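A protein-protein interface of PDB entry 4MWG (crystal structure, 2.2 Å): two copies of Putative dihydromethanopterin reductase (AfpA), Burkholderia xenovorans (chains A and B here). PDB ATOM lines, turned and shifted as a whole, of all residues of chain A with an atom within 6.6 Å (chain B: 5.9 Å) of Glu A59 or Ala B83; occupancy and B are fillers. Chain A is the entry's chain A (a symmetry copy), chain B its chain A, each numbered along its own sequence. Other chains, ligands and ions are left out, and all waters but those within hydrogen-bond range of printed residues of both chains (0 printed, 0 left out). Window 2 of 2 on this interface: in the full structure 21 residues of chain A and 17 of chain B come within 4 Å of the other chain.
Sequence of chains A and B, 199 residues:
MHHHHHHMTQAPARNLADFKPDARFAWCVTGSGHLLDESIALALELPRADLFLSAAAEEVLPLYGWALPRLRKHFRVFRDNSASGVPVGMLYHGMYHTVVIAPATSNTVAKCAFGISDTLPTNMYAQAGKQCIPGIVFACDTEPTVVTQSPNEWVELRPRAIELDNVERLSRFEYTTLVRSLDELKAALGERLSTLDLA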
ATOM      1  N   SER A  54      12.836  -7.676  16.477  1.00  0.00           N
ATOM      2  CA  SER A  54      13.973  -8.501  16.890  1.00  0.00           C
ATOM      3  C   SER A  54      15.253  -7.672  16.758  1.00  0.00           C
ATOM      4  O   SER A  54      15.252  -6.615  16.101  1.00  0.00           O
ATOM      5  CB  SER A  54      14.083  -9.772  16.046  1.00  0.00           C
ATOM      6  OG  SER A  54      14.453  -9.457  14.717  1.00  0.00           O
ATOM      7  N   ALA A  55      16.343  -8.139  17.368  1.00  0.00           N
ATOM      8  CA  ALA A  55      17.634  -7.470  17.212  1.00  0.00           C
ATOM      9  C   ALA A  55      18.070  -7.444  15.741  1.00  0.00           C
ATOM     10  O   ALA A  55      18.585  -6.439  15.265  1.00  0.00           O
ATOM     11  CB  ALA A  55      18.693  -8.147  18.070  1.00  0.00           C
ATOM     12  N   ALA A  56      17.830  -8.529  15.003  1.00  0.00           N
ATOM     13  CA  ALA A  56      18.249  -8.567  13.603  1.00  0.00           C
ATOM     14  C   ALA A  56      17.398  -7.621  12.746  1.00  0.00           C
ATOM     15  O   ALA A  56      17.886  -7.063  11.772  1.00  0.00           O
ATOM     16  CB  ALA A  56      18.187 -10.000  13.040  1.00  0.00           C
ATOM     17  N   ALA A  57      16.134  -7.440  13.115  1.00  0.00           N
ATOM     18  CA  ALA A  57      15.264  -6.507  12.396  1.00  0.00           C
ATOM     19  C   ALA A  57      15.811  -5.090  12.530  1.00  0.00           C
ATOM     20  O   ALA A  57      15.816  -4.311  11.577  1.00  0.00           O
ATOM     21  CB  ALA A  57      13.831  -6.582  12.924  1.00  0.00           C
ATOM     22  N   GLU A  58      16.311  -4.794  13.722  1.00  0.00           N
ATOM     23  CA  GLU A  58      16.855  -3.493  14.037  1.00  0.00           C
ATOM     24  C   GLU A  58      18.081  -3.175  13.183  1.00  0.00           C
ATOM     25  O   GLU A  58      18.335  -2.013  12.865  1.00  0.00           O
ATOM     26  CB  GLU A  58      17.187  -3.426  15.528  1.00  0.00           C
ATOM     27  CG  GLU A  58      17.783  -2.130  15.974  1.00  0.00           C
ATOM     28  CD  GLU A  58      17.491  -1.827  17.428  1.00  0.00           C
ATOM     29  OE1 GLU A  58      17.838  -0.716  17.878  1.00  0.00           O
ATOM     30  OE2 GLU A  58      16.908  -2.686  18.114  1.00  0.00           O
ATOM     31  N   GLU A  59      18.821  -4.203  12.774  1.00  0.00           N
ATOM     32  CA  GLU A  59      19.982  -3.995  11.899  1.00  0.00           C
ATOM     33  C   GLU A  59      19.595  -3.991  10.422  1.00  0.00           C
ATOM     34  O   GLU A  59      20.200  -3.306   9.604  1.00  0.00           O
ATOM     35  CB  GLU A  59      21.030  -5.073  12.140  1.00  0.00           C
ATOM     36  CG  GLU A  59      21.238  -5.378  13.607  1.00  0.00           C
ATOM     37  CD  GLU A  59      22.273  -6.461  13.829  1.00  0.00           C
ATOM     38  OE1 GLU A  59      22.739  -7.047  12.827  1.00  0.00           O
ATOM     39  OE2 GLU A  59      22.621  -6.721  15.002  1.00  0.00           O
ATOM     40  N   VAL A  60      18.578  -4.763  10.084  1.00  0.00           N
ATOM     41  CA  VAL A  60      18.183  -4.938   8.695  1.00  0.00           C
ATOM     42  C   VAL A  60      17.298  -3.804   8.194  1.00  0.00           C
ATOM     43  O   VAL A  60      17.478  -3.314   7.074  1.00  0.00           O
ATOM     44  CB  VAL A  60      17.436  -6.291   8.507  1.00  0.00           C
ATOM     45  CG1 VAL A  60      16.562  -6.282   7.258  1.00  0.00           C
ATOM     46  CG2 VAL A  60      18.430  -7.438   8.469  1.00  0.00           C
ATOM     47  N   LEU A  61      16.327  -3.407   9.015  1.00  0.00           N
ATOM     48  CA  LEU A  61      15.361  -2.386   8.606  1.00  0.00           C
ATOM     49  C   LEU A  61      15.976  -1.102   8.022  1.00  0.00           C
ATOM     50  O   LEU A  61      15.462  -0.594   7.023  1.00  0.00           O
ATOM     51  CB  LEU A  61      14.450  -2.038   9.785  1.00  0.00           C
ATOM     52  CG  LEU A  61      13.248  -2.956   9.977  1.00  0.00           C
ATOM     53  CD1 LEU A  61      12.732  -2.940  11.409  1.00  0.00           C
ATOM     54  CD2 LEU A  61      12.150  -2.506   9.048  1.00  0.00           C
ATOM     55  N   PRO A  62      17.062  -0.561   8.630  1.00  0.00           N
ATOM     56  CA  PRO A  62      17.641   0.658   8.042  1.00  0.00           C
ATOM     57  C   PRO A  62      18.136   0.460   6.615  1.00  0.00           C
ATOM     58  O   PRO A  62      18.120   1.403   5.821  1.00  0.00           O
ATOM     59  CB  PRO A  62      18.828   0.970   8.964  1.00  0.00           C
ATOM     60  CG  PRO A  62      18.489   0.336  10.250  1.00  0.00           C
ATOM     61  CD  PRO A  62      17.714  -0.902   9.906  1.00  0.00           C
ATOM     62  N   LEU A  63      18.581  -0.752   6.303  1.00  0.00           N
ATOM     63  CA  LEU A  63      19.143  -1.035   4.988  1.00  0.00           C
ATOM     64  C   LEU A  63      18.062  -1.048   3.914  1.00  0.00           C
ATOM     65  O   LEU A  63      18.360  -0.999   2.719  1.00  0.00           O
ATOM     66  CB  LEU A  63      19.887  -2.366   5.007  1.00  0.00           C
ATOM     67  CG  LEU A  63      21.192  -2.383   5.802  1.00  0.00           C
ATOM     68  CD1 LEU A  63      21.631  -3.818   6.091  1.00  0.00           C
ATOM     69  CD2 LEU A  63      22.276  -1.634   5.041  1.00  0.00           C
ATOM     70  N   ASP B  80      31.136 -12.508  14.466  1.00  0.00           N
ATOM     71  CA  ASP B  80      29.713 -12.504  14.685  1.00  0.00           C
ATOM     72  C   ASP B  80      29.277 -11.243  15.416  1.00  0.00           C
ATOM     73  O   ASP B  80      28.776 -11.319  16.533  1.00  0.00           O
ATOM     74  CB  ASP B  80      29.339 -13.745  15.497  1.00  0.00           C
ATOM     75  CG  ASP B  80      27.875 -14.125  15.355  1.00  0.00           C
ATOM     76  OD1 ASP B  80      27.053 -13.245  14.980  1.00  0.00           O
ATOM     77  OD2 ASP B  80      27.567 -15.312  15.622  1.00  0.00           O
ATOM     78  N   ASN B  81      29.491 -10.084  14.808  1.00  0.00           N
ATOM     79  CA  ASN B  81      29.118  -8.838  15.464  1.00  0.00           C
ATOM     80  C   ASN B  81      27.944  -8.178  14.753  1.00  0.00           C
ATOM     81  O   ASN B  81      27.917  -6.963  14.550  1.00  0.00           O
ATOM     82  CB  ASN B  81      30.315  -7.879  15.562  1.00  0.00           C
ATOM     83  CG  ASN B  81      31.077  -7.753  14.259  1.00  0.00           C
ATOM     84  OD1 ASN B  81      30.516  -7.938  13.176  1.00  0.00           O
ATOM     85  ND2 ASN B  81      32.366  -7.436  14.356  1.00  0.00           N
ATOM     86  N   SER B  82      26.977  -9.010  14.378  1.00  0.00           N
ATOM     87  CA  SER B  82      25.679  -8.537  13.912  1.00  0.00           C
ATOM     88  C   SER B  82      24.636  -9.641  14.080  1.00  0.00           C
ATOM     89  O   SER B  82      24.880 -10.801  13.735  1.00  0.00           O
ATOM     90  CB  SER B  82      25.745  -8.078  12.451  1.00  0.00           C
ATOM     91  OG  SER B  82      25.750  -9.180  11.562  1.00  0.00           O
ATOM     92  N   ALA B  83      23.482  -9.273  14.630  1.00  0.00           N
ATOM     93  CA  ALA B  83      22.367 -10.202  14.792  1.00  0.00           C
ATOM     94  C   ALA B  83      21.874 -10.687  13.424  1.00  0.00           C
ATOM     95  O   ALA B  83      21.485 -11.850  13.262  1.00  0.00           O
ATOM     96  CB  ALA B  83      21.236  -9.542  15.575  1.00  0.00           C
ATOM     97  N   SER B  84      21.921  -9.787  12.442  1.00  0.00           N
ATOM     98  CA  SER B  84      21.479 -10.073  11.080  1.00  0.00           C
ATOM     99  C   SER B  84      22.436 -11.002  10.331  1.00  0.00           C
ATOM    100  O   SER B  84      22.014 -11.744   9.438  1.00  0.00           O
ATOM    101  CB  SER B  84      21.314  -8.769  10.296  1.00  0.00           C
ATOM    102  OG  SER B  84      22.563  -8.117  10.117  1.00  0.00           O
ATOM    103  N   GLY B  85      23.718 -10.957  10.696  1.00  0.00           N
ATOM    104  CA  GLY B  85      24.742 -11.727  10.008  1.00  0.00           C
ATOM    105  C   GLY B  85      25.162 -11.060   8.708  1.00  0.00           C
ATOM    106  O   GLY B  85      25.178 -11.687   7.651  1.00  0.00           O
ATOM    107  N   VAL B  86      25.513  -9.780   8.792  1.00  0.00           N
ATOM    108  CA  VAL B  86      25.886  -8.973   7.620  1.00  0.00           C
ATOM    109  C   VAL B  86      26.922  -9.582   6.631  1.00  0.00           C
ATOM    110  O   VAL B  86      26.799  -9.369   5.418  1.00  0.00           O
ATOM    111  CB  VAL B  86      26.401  -7.592   8.081  1.00  0.00           C
ATOM    112  CG1 VAL B  86      26.597  -6.667   6.891  1.00  0.00           C
ATOM    113  CG2 VAL B  86      25.422  -6.977   9.066  1.00  0.00           C
ATOM    114  N   SER B 117      18.932 -20.143  12.559  1.00  0.00           N
ATOM    115  CA  SER B 117      20.148 -19.460  12.127  1.00  0.00           C
ATOM    116  C   SER B 117      20.333 -18.129  12.877  1.00  0.00           C
ATOM    117  O   SER B 117      20.121 -17.066  12.313  1.00  0.00           O
ATOM    118  CB  SER B 117      20.105 -19.226  10.612  1.00  0.00           C
ATOM    119  OG  SER B 117      18.934 -18.517  10.243  1.00  0.00           O
ATOM    120  N   ASP B 118      20.724 -18.191  14.154  1.00  0.00           N
ATOM    121  CA  ASP B 118      20.880 -16.951  14.934  1.00  0.00           C
ATOM    122  C   ASP B 118      22.351 -16.765  15.355  1.00  0.00           C
ATOM    123  O   ASP B 118      22.643 -16.086  16.328  1.00  0.00           O
ATOM    124  CB  ASP B 118      19.919 -16.933  16.161  1.00  0.00           C
ATOM    125  CG  ASP B 118      20.156 -18.121  17.134  1.00  0.00           C
ATOM    126  OD1 ASP B 118      21.110 -18.882  16.906  1.00  0.00           O
ATOM    127  OD2 ASP B 118      19.418 -18.264  18.146  1.00  0.00           O
ATOM    128  N   ASN B 123      23.887 -19.100  10.208  1.00  0.00           N
ATOM    129  CA  ASN B 123      23.382 -18.247   9.128  1.00  0.00           C
ATOM    130  C   ASN B 123      24.093 -18.523   7.793  1.00  0.00           C
ATOM    131  O   ASN B 123      23.445 -18.626   6.755  1.00  0.00           O
ATOM    132  CB  ASN B 123      23.520 -16.761   9.489  1.00  0.00           C
ATOM    133  CG  ASN B 123      22.259 -16.191  10.130  1.00  0.00           C
ATOM    134  OD1 ASN B 123      21.155 -16.337   9.595  1.00  0.00           O
ATOM    135  ND2 ASN B 123      22.419 -15.539  11.279  1.00  0.00           N
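Glu A59 touches just these residues of chain B: Ser B82, Ala B83 and Ser B84. Of the printed residues of chain A, Ala B83 touches Ala A55, Ala A56 and Glu A59. Of the printed residues of chain A, Ser B84 touches Ala A56, Glu A59 and Val A60. Printed residues of chain A within 4 Å of Ser B82: Glu A59. Of the printed residues of chain B, Val A60 touches Ser B84 (3.7 Å). Of the printed residues of chain B, Ala A55 touches Ala B83 (3.8 Å). Val B86 touches none of the printed residues of chain A. The nearest residue of chain B that does not touch Glu A59 is Gly B85 (4.6 Å). The nearest printed residue of chain A that does not touch Ser B84 is Ala A55 (5.5 Å).
C of Ala A55 touches CB of Ala B83, at 3.8 Å. Ala B83 touches Ala A56. CB of Ala A56 touches N of Ser B84 (3.8 Å). Glu A59 touches Ser B82. Ser B84 touches Val A60 (CB to CG2, 3.7 Å).
OE2 of Glu A59 sits at hydrogen-bond distance from N of Ala B83. N of Ser B84 is in hydrogen-bond range of OE1 of Glu A59 (2.9 Å).
No position is printed for both chains. Of the 7 pairs that touch across the chains among the printed residues, none has its exchanged pair printed and touching as well.
OG of Ser B82 is in hydrogen-bond range of N of Gly B85. The backbone NH (N) of Val B86 is in hydrogen-bond range of the side-chain hydroxyl (OG) of Ser B82, 2.8 Å away.
Of the 10 printed residues of chain B, 3 touch a printed residue of chain A. Printed residues of chain A that touch a printed residue of chain B: Ala A55, Ala A56, Glu A59 and Val A60. Hydrophobic or aromatic side chains of chain A that line the printed part of chain B: Ala A55, Ala A56 and Val A60. Among the printed residues, 7 pairs touch across the chains.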
